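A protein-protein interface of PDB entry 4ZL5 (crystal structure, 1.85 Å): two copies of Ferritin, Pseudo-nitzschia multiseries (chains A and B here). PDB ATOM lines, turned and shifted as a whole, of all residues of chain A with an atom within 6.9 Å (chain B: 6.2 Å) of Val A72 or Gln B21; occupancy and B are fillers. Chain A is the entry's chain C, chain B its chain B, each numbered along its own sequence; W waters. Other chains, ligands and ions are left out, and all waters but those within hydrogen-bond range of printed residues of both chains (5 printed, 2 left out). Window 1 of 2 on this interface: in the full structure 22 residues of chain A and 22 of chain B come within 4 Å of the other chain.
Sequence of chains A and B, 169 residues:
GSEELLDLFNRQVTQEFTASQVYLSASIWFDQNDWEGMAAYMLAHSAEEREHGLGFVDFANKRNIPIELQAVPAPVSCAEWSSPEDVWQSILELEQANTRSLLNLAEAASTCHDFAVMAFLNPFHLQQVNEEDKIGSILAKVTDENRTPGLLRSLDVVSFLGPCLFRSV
Printed residues of chain A within 4 Å of Pro B75: Leu A69.
Of the printed residues of chain A, Leu B24 touches Phe A17 (3.6 Å), Leu A54 (3.7 Å) and Leu A69 (3.9 Å).
Thr A14 touches none of the printed residues of chain B.
Pro A73 touches none of the printed residues of chain B.
The nearest residue of chain B that does not touch Val A72 is Gln B70 (4.5 Å).
The nearest printed residue of chain A that does not touch Phe B17 is Val A72 (7.3 Å).
The backbone NH (N) of Val B72 sits at hydrogen-bond distance from the backbone carbonyl oxygen (O) of Val A72 (2.9 Å).
The side-chain hydroxyl (OG) of Ser B46 is in hydrogen-bond range of the guanidinium group (NH2) of Arg A50, at 2.8 Å.
Hydrophobic or aromatic side chains of chain B that line the printed part of chain A: Phe B17, Leu B24, Ala B71, Val B72, Ala B74 and Pro B75.
Printed residues of chain A that touch a printed residue of chain B: Phe A17, Gln A21, Arg A50, Leu A54, Leu A69, Gln A70, Ala A71, Val A72 and Ala A74.
Hydrophobic or aromatic side chains of chain A that line the printed part of chain B: Phe A17, Leu A54, Leu A69, Ala A71, Val A72 and Ala A74.
Among the printed residues, 18 pairs touch across the chains.
Among the printed residues, no Asp or Glu carboxylate lies within 4 Å of a Lys or Arg side-chain nitrogen of the other chain.
Gln A21 touches Phe B17, but with the chains exchanged Phe A17 does not touch Gln B21 (4.1 Å).
Gln A70 touches Ala B74, and with the chains exchanged Ala A74 touches Gln B70.
Ala A71 touches Ala B74, and with the chains exchanged Ala A74 touches Ala B71.
Val A72 touches Gln B21, but with the chains exchanged Gln A21 does not touch Val B72 (4.2 Å).
Positions printed for both chains: 17, 18, 19, 20, 21, 22, 70, 71, 72, 73, 74 and 75.
Of the 18 pairs that touch across the chains among the printed residues, 7 have their exchanged pair printed and touching as well.
The side-chain hydroxyl (OG) of Ser B20 lies within hydrogen-bond range of the backbone carbonyl oxygen (O) of Ser B46, at 2.8 Å.
Among the printed residues, merely in contact across the chains: Val A72 with Ala B71, Ala A71 with Val B72, Phe A17 with Leu B24, Leu A69 with Ala B74, Ala A71 with Ala B74, Ala A74 with Ala B71, Leu A69 with Gln B21, Leu A54 with Leu B24, Leu A69 with Ser B25, Leu A69 with Pro B75, Val A72 with Gln B21, Leu A69 with Leu B24, Arg A50 with Ser B20, Gln A70 with Ala B74, Gln A21 with Phe B17 and Ala A74 with Gln B70.
Water W5 lies within hydrogen-bond range of O of Pro B75 and O of Leu A69.
Water W4 lies within hydrogen-bond range of the side-chain amide nitrogen (NE2) of Gln B21 (2.7 Å), the side-chain hydroxyl (OG) of Ser B20 (2.9 Å), the guanidinium group (NE) of Arg A50 (3.1 Å) and the side-chain hydroxyl (OG) of Ser B46 (3.5 Å).
Water W2 lies within hydrogen-bond range of O of Gln A70 (2.8 Å) and OE1 of Gln B21 (3.0 Å).
Water W3 bridges O of Gln B70 (2.9 Å) and NE2 of Gln A21 (3.2 Å).
Water W1 lies within hydrogen-bond range of the backbone NH of Leu A69 (2.9 Å) and the side-chain hydroxyl of Ser B25 (3.3 Å).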
ATOM      1  N   VAL A  13     -17.514 -14.397 -28.031  1.00  0.00           N
ATOM      2  CA  VAL A  13     -18.482 -13.326 -28.185  1.00  0.00           C
ATOM      3  C   VAL A  13     -19.501 -13.510 -27.101  1.00  0.00           C
ATOM      4  O   VAL A  13     -19.850 -12.561 -26.376  1.00  0.00           O
ATOM      5  CB  VAL A  13     -19.106 -13.265 -29.598  1.00  0.00           C
ATOM      6  CG1 VAL A  13     -20.271 -12.252 -29.698  1.00  0.00           C
ATOM      7  CG2 VAL A  13     -18.036 -12.933 -30.619  1.00  0.00           C
ATOM      8  N   THR A  14     -19.978 -14.732 -26.981  1.00  0.00           N
ATOM      9  CA  THR A  14     -21.054 -14.983 -26.004  1.00  0.00           C
ATOM     10  C   THR A  14     -20.566 -14.668 -24.590  1.00  0.00           C
ATOM     11  O   THR A  14     -21.309 -14.106 -23.775  1.00  0.00           O
ATOM     12  CB  THR A  14     -21.527 -16.415 -26.140  1.00  0.00           C
ATOM     13  OG1 THR A  14     -21.917 -16.637 -27.499  1.00  0.00           O
ATOM     14  CG2 THR A  14     -22.695 -16.685 -25.159  1.00  0.00           C
ATOM     15  N   PHE A  17     -20.522 -10.852 -23.895  1.00  0.00           N
ATOM     16  CA  PHE A  17     -21.855 -10.323 -23.654  1.00  0.00           C
ATOM     17  C   PHE A  17     -22.475 -10.835 -22.346  1.00  0.00           C
ATOM     18  O   PHE A  17     -23.119 -10.117 -21.666  1.00  0.00           O
ATOM     19  CB  PHE A  17     -22.765 -10.642 -24.854  1.00  0.00           C
ATOM     20  CG  PHE A  17     -22.364  -9.922 -26.144  1.00  0.00           C
ATOM     21  CD1 PHE A  17     -21.532  -8.807 -26.142  1.00  0.00           C
ATOM     22  CD2 PHE A  17     -22.777 -10.396 -27.376  1.00  0.00           C
ATOM     23  CE1 PHE A  17     -21.189  -8.137 -27.299  1.00  0.00           C
ATOM     24  CE2 PHE A  17     -22.435  -9.715 -28.544  1.00  0.00           C
ATOM     25  CZ  PHE A  17     -21.634  -8.580 -28.500  1.00  0.00           C
ATOM     26  N   THR A  18     -22.202 -12.088 -21.977  1.00  0.00           N
ATOM     27  CA  THR A  18     -22.628 -12.620 -20.726  1.00  0.00           C
ATOM     28  C   THR A  18     -22.003 -11.815 -19.570  1.00  0.00           C
ATOM     29  O   THR A  18     -22.713 -11.453 -18.624  1.00  0.00           O
ATOM     30  CB  THR A  18     -22.240 -14.101 -20.652  1.00  0.00           C
ATOM     31  OG1 THR A  18     -22.901 -14.837 -21.695  1.00  0.00           O
ATOM     32  CG2 THR A  18     -22.472 -14.749 -19.271  1.00  0.00           C
ATOM     33  N   ALA A  19     -20.697 -11.528 -19.666  1.00  0.00           N
ATOM     34  CA  ALA A  19     -19.968 -10.756 -18.686  1.00  0.00           C
ATOM     35  C   ALA A  19     -20.532  -9.340 -18.647  1.00  0.00           C
ATOM     36  O   ALA A  19     -20.764  -8.762 -17.565  1.00  0.00           O
ATOM     37  CB  ALA A  19     -18.468 -10.752 -19.026  1.00  0.00           C
ATOM     38  N   SER A  20     -20.853  -8.791 -19.803  1.00  0.00           N
ATOM     39  CA  SER A  20     -21.520  -7.479 -19.837  1.00  0.00           C
ATOM     40  C   SER A  20     -22.778  -7.508 -18.993  1.00  0.00           C
ATOM     41  O   SER A  20     -23.027  -6.606 -18.195  1.00  0.00           O
ATOM     42  CB  SER A  20     -21.815  -6.990 -21.255  1.00  0.00           C
ATOM     43  OG  SER A  20     -22.506  -5.749 -21.250  1.00  0.00           O
ATOM     44  N   GLN A  21     -23.599  -8.535 -19.145  1.00  0.00           N
ATOM     45  CA  GLN A  21     -24.790  -8.601 -18.356  1.00  0.00           C
ATOM     46  C   GLN A  21     -24.600  -8.770 -16.865  1.00  0.00           C
ATOM     47  O   GLN A  21     -25.385  -8.227 -16.075  1.00  0.00           O
ATOM     48  CB  GLN A  21     -25.734  -9.687 -18.867  1.00  0.00           C
ATOM     49  CG  GLN A  21     -26.397  -9.344 -20.160  1.00  0.00           C
ATOM     50  CD  GLN A  21     -27.438  -8.217 -20.017  1.00  0.00           C
ATOM     51  OE1 GLN A  21     -27.087  -7.067 -20.211  1.00  0.00           O
ATOM     52  NE2 GLN A  21     -28.695  -8.549 -19.723  1.00  0.00           N
ATOM     53  N   VAL A  22     -23.665  -9.630 -16.476  1.00  0.00           N
ATOM     54  CA  VAL A  22     -23.348  -9.845 -15.078  1.00  0.00           C
ATOM     55  C   VAL A  22     -22.849  -8.534 -14.437  1.00  0.00           C
ATOM     56  O   VAL A  22     -23.310  -8.130 -13.404  1.00  0.00           O
ATOM     57  CB  VAL A  22     -22.289 -10.952 -14.914  1.00  0.00           C
ATOM     58  CG1 VAL A  22     -21.878 -11.046 -13.447  1.00  0.00           C
ATOM     59  CG2 VAL A  22     -22.826 -12.328 -15.380  1.00  0.00           C
ATOM     60  N   ARG A  50     -19.060  -5.277 -23.412  1.00  0.00           N
ATOM     61  CA  ARG A  50     -19.781  -5.246 -24.680  1.00  0.00           C
ATOM     62  C   ARG A  50     -18.859  -4.809 -25.834  1.00  0.00           C
ATOM     63  O   ARG A  50     -18.884  -5.440 -26.888  1.00  0.00           O
ATOM     64  CB  ARG A  50     -21.021  -4.341 -24.649  1.00  0.00           C
ATOM     65  CG  ARG A  50     -21.829  -4.402 -25.927  1.00  0.00           C
ATOM     66  CD  ARG A  50     -23.294  -3.973 -25.773  1.00  0.00           C
ATOM     67  NE  ARG A  50     -24.006  -4.023 -27.070  1.00  0.00           N
ATOM     68  CZ  ARG A  50     -23.906  -3.025 -27.970  1.00  0.00           C
ATOM     69  NH1 ARG A  50     -23.190  -1.974 -27.684  1.00  0.00           N
ATOM     70  NH2 ARG A  50     -24.496  -3.084 -29.137  1.00  0.00           N
ATOM     71  N   LEU A  54     -17.991  -6.758 -29.329  1.00  0.00           N
ATOM     72  CA  LEU A  54     -18.100  -6.163 -30.638  1.00  0.00           C
ATOM     73  C   LEU A  54     -16.802  -6.207 -31.434  1.00  0.00           C
ATOM     74  O   LEU A  54     -16.829  -6.351 -32.660  1.00  0.00           O
ATOM     75  CB  LEU A  54     -18.562  -4.763 -30.497  1.00  0.00           C
ATOM     76  CG  LEU A  54     -19.970  -4.578 -29.905  1.00  0.00           C
ATOM     77  CD1 LEU A  54     -20.138  -3.068 -29.775  1.00  0.00           C
ATOM     78  CD2 LEU A  54     -21.052  -5.220 -30.771  1.00  0.00           C
ATOM     79  N   LEU A  69     -25.083 -15.245 -33.221  1.00  0.00           N
ATOM     80  CA  LEU A  69     -25.275 -14.753 -31.873  1.00  0.00           C
ATOM     81  C   LEU A  69     -26.034 -15.742 -31.035  1.00  0.00           C
ATOM     82  O   LEU A  69     -27.077 -16.260 -31.480  1.00  0.00           O
ATOM     83  CB  LEU A  69     -26.016 -13.413 -31.853  1.00  0.00           C
ATOM     84  CG  LEU A  69     -25.162 -12.299 -32.506  1.00  0.00           C
ATOM     85  CD1 LEU A  69     -25.943 -11.006 -32.576  1.00  0.00           C
ATOM     86  CD2 LEU A  69     -23.865 -12.099 -31.744  1.00  0.00           C
ATOM     87  N   GLN A  70     -25.515 -16.050 -29.854  1.00  0.00           N
ATOM     88  CA  GLN A  70     -26.221 -16.952 -28.958  1.00  0.00           C
ATOM     89  C   GLN A  70     -26.985 -16.179 -27.922  1.00  0.00           C
ATOM     90  O   GLN A  70     -26.831 -14.957 -27.757  1.00  0.00           O
ATOM     91  CB  GLN A  70     -25.233 -17.972 -28.354  1.00  0.00           C
ATOM     92  CG  GLN A  70     -24.512 -18.780 -29.460  1.00  0.00           C
ATOM     93  CD  GLN A  70     -25.480 -19.758 -30.235  1.00  0.00           C
ATOM     94  OE1 GLN A  70     -26.615 -20.046 -29.805  1.00  0.00           O
ATOM     95  NE2 GLN A  70     -25.045 -20.226 -31.381  1.00  0.00           N
ATOM     96  N   ALA A  71     -27.817 -16.880 -27.151  1.00  0.00           N
ATOM     97  CA  ALA A  71     -28.429 -16.276 -26.048  1.00  0.00           C
ATOM     98  C   ALA A  71     -27.427 -15.710 -25.047  1.00  0.00           C
ATOM     99  O   ALA A  71     -26.370 -16.238 -24.856  1.00  0.00           O
ATOM    100  CB  ALA A  71     -29.351 -17.284 -25.297  1.00  0.00           C
ATOM    101  N   VAL A  72     -27.871 -14.694 -24.349  1.00  0.00           N
ATOM    102  CA  VAL A  72     -27.185 -14.124 -23.229  1.00  0.00           C
ATOM    103  C   VAL A  72     -27.967 -14.539 -21.982  1.00  0.00           C
ATOM    104  O   VAL A  72     -29.017 -14.010 -21.744  1.00  0.00           O
ATOM    105  CB  VAL A  72     -27.131 -12.588 -23.356  1.00  0.00           C
ATOM    106  CG1 VAL A  72     -26.243 -12.062 -22.266  1.00  0.00           C
ATOM    107  CG2 VAL A  72     -26.562 -12.240 -24.760  1.00  0.00           C
ATOM    108  N   PRO A  73     -27.421 -15.477 -21.194  1.00  0.00           N
ATOM    109  CA  PRO A  73     -28.153 -15.943 -20.019  1.00  0.00           C
ATOM    110  C   PRO A  73     -28.464 -14.894 -18.972  1.00  0.00           C
ATOM    111  O   PRO A  73     -27.764 -13.854 -18.871  1.00  0.00           O
ATOM    112  CB  PRO A  73     -27.259 -17.029 -19.445  1.00  0.00           C
ATOM    113  CG  PRO A  73     -25.869 -16.802 -20.003  1.00  0.00           C
ATOM    114  CD  PRO A  73     -26.050 -16.017 -21.272  1.00  0.00           C
ATOM    115  N   ALA A  74     -29.544 -15.093 -18.243  1.00  0.00           N
ATOM    116  CA  ALA A  74     -29.881 -14.282 -17.064  1.00  0.00           C
ATOM    117  C   ALA A  74     -28.793 -14.385 -15.983  1.00  0.00           C
ATOM    118  O   ALA A  74     -28.350 -15.510 -15.635  1.00  0.00           O
ATOM    119  CB  ALA A  74     -31.210 -14.705 -16.458  1.00  0.00           C
ATOM    120  N   PRO A  75     -28.341 -13.244 -15.460  1.00  0.00           N
ATOM    121  CA  PRO A  75     -27.330 -13.264 -14.426  1.00  0.00           C
ATOM    122  C   PRO A  75     -28.005 -13.840 -13.186  1.00  0.00           C
ATOM    123  O   PRO A  75     -29.135 -13.528 -12.920  1.00  0.00           O
ATOM    124  CB  PRO A  75     -26.969 -11.781 -14.238  1.00  0.00           C
ATOM    125  CG  PRO A  75     -27.277 -11.169 -15.534  1.00  0.00           C
ATOM    126  CD  PRO A  75     -28.468 -11.915 -16.089  1.00  0.00           C
ATOM    127  N   GLU B  16     -35.744  -4.074 -24.871  1.00  0.00           N
ATOM    128  CA  GLU B  16     -34.713  -3.184 -25.403  1.00  0.00           C
ATOM    129  C   GLU B  16     -33.430  -3.934 -25.637  1.00  0.00           C
ATOM    130  O   GLU B  16     -32.805  -3.734 -26.680  1.00  0.00           O
ATOM    131  CB  GLU B  16     -34.432  -2.026 -24.434  1.00  0.00           C
ATOM    132  CG  GLU B  16     -35.604  -1.132 -24.138  1.00  0.00           C
ATOM    133  CD  GLU B  16     -36.128  -0.432 -25.391  1.00  0.00           C
ATOM    134  OE1 GLU B  16     -35.360  -0.264 -26.349  1.00  0.00           O
ATOM    135  OE2 GLU B  16     -37.325  -0.108 -25.407  1.00  0.00           O
ATOM    136  N   PHE B  17     -33.031  -4.809 -24.695  1.00  0.00           N
ATOM    137  CA  PHE B  17     -31.843  -5.571 -24.879  1.00  0.00           C
ATOM    138  C   PHE B  17     -31.974  -6.581 -26.025  1.00  0.00           C
ATOM    139  O   PHE B  17     -31.004  -6.836 -26.760  1.00  0.00           O
ATOM    140  CB  PHE B  17     -31.418  -6.228 -23.590  1.00  0.00           C
ATOM    141  CG  PHE B  17     -30.919  -5.265 -22.500  1.00  0.00           C
ATOM    142  CD1 PHE B  17     -30.503  -3.968 -22.773  1.00  0.00           C
ATOM    143  CD2 PHE B  17     -30.958  -5.654 -21.168  1.00  0.00           C
ATOM    144  CE1 PHE B  17     -30.068  -3.121 -21.773  1.00  0.00           C
ATOM    145  CE2 PHE B  17     -30.531  -4.806 -20.139  1.00  0.00           C
ATOM    146  CZ  PHE B  17     -30.083  -3.525 -20.460  1.00  0.00           C
ATOM    147  N   THR B  18     -33.137  -7.201 -26.123  1.00  0.00           N
ATOM    148  CA  THR B  18     -33.471  -8.126 -27.202  1.00  0.00           C
ATOM    149  C   THR B  18     -33.337  -7.372 -28.554  1.00  0.00           C
ATOM    150  O   THR B  18     -32.685  -7.895 -29.477  1.00  0.00           O
ATOM    151  CB  THR B  18     -34.873  -8.741 -27.065  1.00  0.00           C
ATOM    152  OG1 THR B  18     -34.962  -9.573 -25.911  1.00  0.00           O
ATOM    153  CG2 THR B  18     -35.265  -9.550 -28.291  1.00  0.00           C
ATOM    154  N   ALA B  19     -33.934  -6.168 -28.652  1.00  0.00           N
ATOM    155  CA  ALA B  19     -33.770  -5.362 -29.873  1.00  0.00           C
ATOM    156  C   ALA B  19     -32.320  -5.036 -30.141  1.00  0.00           C
ATOM    157  O   ALA B  19     -31.890  -5.114 -31.303  1.00  0.00           O
ATOM    158  CB  ALA B  19     -34.609  -4.087 -29.824  1.00  0.00           C
ATOM    159  N   SER B  20     -31.542  -4.726 -29.101  1.00  0.00           N
ATOM    160  CA  SER B  20     -30.124  -4.509 -29.270  1.00  0.00           C
ATOM    161  C   SER B  20     -29.441  -5.668 -29.999  1.00  0.00           C
ATOM    162  O   SER B  20     -28.598  -5.457 -30.941  1.00  0.00           O
ATOM    163  CB  SER B  20     -29.465  -4.200 -27.903  1.00  0.00           C
ATOM    164  OG  SER B  20     -28.164  -3.811 -28.068  1.00  0.00           O
ATOM    165  N   GLN B  21     -29.716  -6.902 -29.570  1.00  0.00           N
ATOM    166  CA  GLN B  21     -29.094  -8.065 -30.182  1.00  0.00           C
ATOM    167  C   GLN B  21     -29.589  -8.286 -31.580  1.00  0.00           C
ATOM    168  O   GLN B  21     -28.840  -8.693 -32.465  1.00  0.00           O
ATOM    169  CB  GLN B  21     -29.363  -9.339 -29.389  1.00  0.00           C
ATOM    170  CG  GLN B  21     -28.664  -9.359 -28.146  1.00  0.00           C
ATOM    171  CD  GLN B  21     -27.189  -9.664 -28.307  1.00  0.00           C
ATOM    172  OE1 GLN B  21     -26.759 -10.856 -28.333  1.00  0.00           O
ATOM    173  NE2 GLN B  21     -26.406  -8.597 -28.200  1.00  0.00           N
ATOM    174  N   VAL B  22     -30.862  -8.010 -31.798  1.00  0.00           N
ATOM    175  CA  VAL B  22     -31.407  -8.122 -33.168  1.00  0.00           C
ATOM    176  C   VAL B  22     -30.707  -7.149 -34.105  1.00  0.00           C
ATOM    177  O   VAL B  22     -30.292  -7.548 -35.200  1.00  0.00           O
ATOM    178  CB  VAL B  22     -32.920  -8.002 -33.234  1.00  0.00           C
ATOM    179  CG1 VAL B  22     -33.448  -8.093 -34.665  1.00  0.00           C
ATOM    180  CG2 VAL B  22     -33.554  -9.191 -32.473  1.00  0.00           C
ATOM    181  N   TYR B  23     -30.584  -5.898 -33.722  1.00  0.00           N
ATOM    182  CA  TYR B  23     -29.854  -4.947 -34.537  1.00  0.00           C
ATOM    183  C   TYR B  23     -28.429  -5.386 -34.756  1.00  0.00           C
ATOM    184  O   TYR B  23     -27.875  -5.208 -35.854  1.00  0.00           O
ATOM    185  CB  TYR B  23     -29.876  -3.555 -33.879  1.00  0.00           C
ATOM    186  CG  TYR B  23     -31.075  -2.722 -34.170  1.00  0.00           C
ATOM    187  CD1 TYR B  23     -31.189  -2.030 -35.353  1.00  0.00           C
ATOM    188  CD2 TYR B  23     -32.082  -2.541 -33.252  1.00  0.00           C
ATOM    189  CE1 TYR B  23     -32.276  -1.208 -35.618  1.00  0.00           C
ATOM    190  CE2 TYR B  23     -33.222  -1.781 -33.550  1.00  0.00           C
ATOM    191  CZ  TYR B  23     -33.270  -1.098 -34.736  1.00  0.00           C
ATOM    192  OH  TYR B  23     -34.253  -0.255 -35.079  1.00  0.00           O
ATOM    193  N   LEU B  24     -27.777  -5.931 -33.716  1.00  0.00           N
ATOM    194  CA  LEU B  24     -26.469  -6.492 -33.918  1.00  0.00           C
ATOM    195  C   LEU B  24     -26.452  -7.612 -34.985  1.00  0.00           C
ATOM    196  O   LEU B  24     -25.530  -7.679 -35.857  1.00  0.00           O
ATOM    197  CB  LEU B  24     -25.849  -6.943 -32.582  1.00  0.00           C
ATOM    198  CG  LEU B  24     -24.405  -7.472 -32.674  1.00  0.00           C
ATOM    199  CD1 LEU B  24     -23.441  -6.463 -33.322  1.00  0.00           C
ATOM    200  CD2 LEU B  24     -23.868  -7.961 -31.318  1.00  0.00           C
ATOM    201  N   SER B  25     -27.426  -8.509 -34.942  1.00  0.00           N
ATOM    202  CA  SER B  25     -27.468  -9.597 -35.927  1.00  0.00           C
ATOM    203  C   SER B  25     -27.677  -9.037 -37.331  1.00  0.00           C
ATOM    204  O   SER B  25     -27.188  -9.591 -38.308  1.00  0.00           O
ATOM    205  CB  SER B  25     -28.599 -10.560 -35.580  1.00  0.00           C
ATOM    206  OG  SER B  25     -28.702 -11.605 -36.527  1.00  0.00           O
ATOM    207  N   ALA B  26     -28.434  -7.949 -37.437  1.00  0.00           N
ATOM    208  CA  ALA B  26     -28.585  -7.269 -38.749  1.00  0.00           C
ATOM    209  C   ALA B  26     -27.260  -6.681 -39.243  1.00  0.00           C
ATOM    210  O   ALA B  26     -26.933  -6.809 -40.453  1.00  0.00           O
ATOM    211  CB  ALA B  26     -29.621  -6.180 -38.671  1.00  0.00           C
ATOM    212  N   SER B  46     -28.055  -0.627 -32.530  1.00  0.00           N
ATOM    213  CA  SER B  46     -27.887  -1.610 -31.504  1.00  0.00           C
ATOM    214  C   SER B  46     -27.441  -0.983 -30.189  1.00  0.00           C
ATOM    215  O   SER B  46     -28.000  -1.276 -29.139  1.00  0.00           O
ATOM    216  CB  SER B  46     -26.825  -2.614 -31.959  1.00  0.00           C
ATOM    217  OG  SER B  46     -26.596  -3.562 -30.948  1.00  0.00           O
ATOM    218  N   GLN B  70     -33.552 -10.609 -17.336  1.00  0.00           N
ATOM    219  CA  GLN B  70     -33.883 -11.855 -18.000  1.00  0.00           C
ATOM    220  C   GLN B  70     -32.874 -12.240 -19.066  1.00  0.00           C
ATOM    221  O   GLN B  70     -31.976 -11.468 -19.425  1.00  0.00           O
ATOM    222  CB  GLN B  70     -35.276 -11.708 -18.588  1.00  0.00           C
ATOM    223  CG  GLN B  70     -36.387 -11.531 -17.581  1.00  0.00           C
ATOM    224  CD  GLN B  70     -36.491 -12.703 -16.584  1.00  0.00           C
ATOM    225  OE1 GLN B  70     -36.927 -12.544 -15.429  1.00  0.00           O
ATOM    226  NE2 GLN B  70     -36.112 -13.904 -17.038  1.00  0.00           N
ATOM    227  N   ALA B  71     -32.950 -13.483 -19.536  1.00  0.00           N
ATOM    228  CA  ALA B  71     -32.120 -13.913 -20.595  1.00  0.00           C
ATOM    229  C   ALA B  71     -32.467 -13.067 -21.790  1.00  0.00           C
ATOM    230  O   ALA B  71     -33.617 -12.772 -21.979  1.00  0.00           O
ATOM    231  CB  ALA B  71     -32.403 -15.389 -20.942  1.00  0.00           C
ATOM    232  N   VAL B  72     -31.488 -12.784 -22.593  1.00  0.00           N
ATOM    233  CA  VAL B  72     -31.712 -12.212 -23.899  1.00  0.00           C
ATOM    234  C   VAL B  72     -31.619 -13.317 -24.936  1.00  0.00           C
ATOM    235  O   VAL B  72     -30.552 -13.884 -25.126  1.00  0.00           O
ATOM    236  CB  VAL B  72     -30.700 -11.122 -24.222  1.00  0.00           C
ATOM    237  CG1 VAL B  72     -31.097 -10.369 -25.501  1.00  0.00           C
ATOM    238  CG2 VAL B  72     -30.626 -10.141 -23.049  1.00  0.00           C
ATOM    239  N   PRO B  73     -32.727 -13.607 -25.616  1.00  0.00           N
ATOM    240  CA  PRO B  73     -32.745 -14.804 -26.494  1.00  0.00           C
ATOM    241  C   PRO B  73     -31.864 -14.646 -27.697  1.00  0.00           C
ATOM    242  O   PRO B  73     -31.581 -13.477 -28.097  1.00  0.00           O
ATOM    243  CB  PRO B  73     -34.224 -14.903 -26.923  1.00  0.00           C
ATOM    244  CG  PRO B  73     -34.767 -13.493 -26.864  1.00  0.00           C
ATOM    245  CD  PRO B  73     -34.063 -12.973 -25.579  1.00  0.00           C
ATOM    246  N   ALA B  74     -31.432 -15.793 -28.255  1.00  0.00           N
ATOM    247  CA  ALA B  74     -30.678 -15.830 -29.540  1.00  0.00           C
ATOM    248  C   ALA B  74     -31.560 -15.237 -30.647  1.00  0.00           C
ATOM    249  O   ALA B  74     -32.721 -15.634 -30.804  1.00  0.00           O
ATOM    250  CB  ALA B  74     -30.225 -17.226 -29.893  1.00  0.00           C
ATOM    251  N   PRO B  75     -31.040 -14.229 -31.383  1.00  0.00           N
ATOM    252  CA  PRO B  75     -31.809 -13.741 -32.546  1.00  0.00           C
ATOM    253  C   PRO B  75     -32.042 -14.841 -33.558  1.00  0.00           C
ATOM    254  O   PRO B  75     -31.135 -15.632 -33.803  1.00  0.00           O
ATOM    255  CB  PRO B  75     -30.877 -12.664 -33.150  1.00  0.00           C
ATOM    256  CG  PRO B  75     -29.961 -12.275 -32.066  1.00  0.00           C
ATOM    257  CD  PRO B  75     -29.763 -13.517 -31.210  1.00  0.00           C
HETATM  258  O   HOH W   1     -26.499 -13.702 -35.197  1.00  0.00           O
HETATM  259  O   HOH W   2     -24.840 -13.092 -28.117  1.00  0.00           O
HETATM  260  O   HOH W   3     -31.916  -8.630 -19.775  1.00  0.00           O
HETATM  261  O   HOH W   4     -26.110  -5.888 -28.418  1.00  0.00           O
HETATM  262  O   HOH W   5     -28.468 -15.490 -33.960  1.00  0.00           O
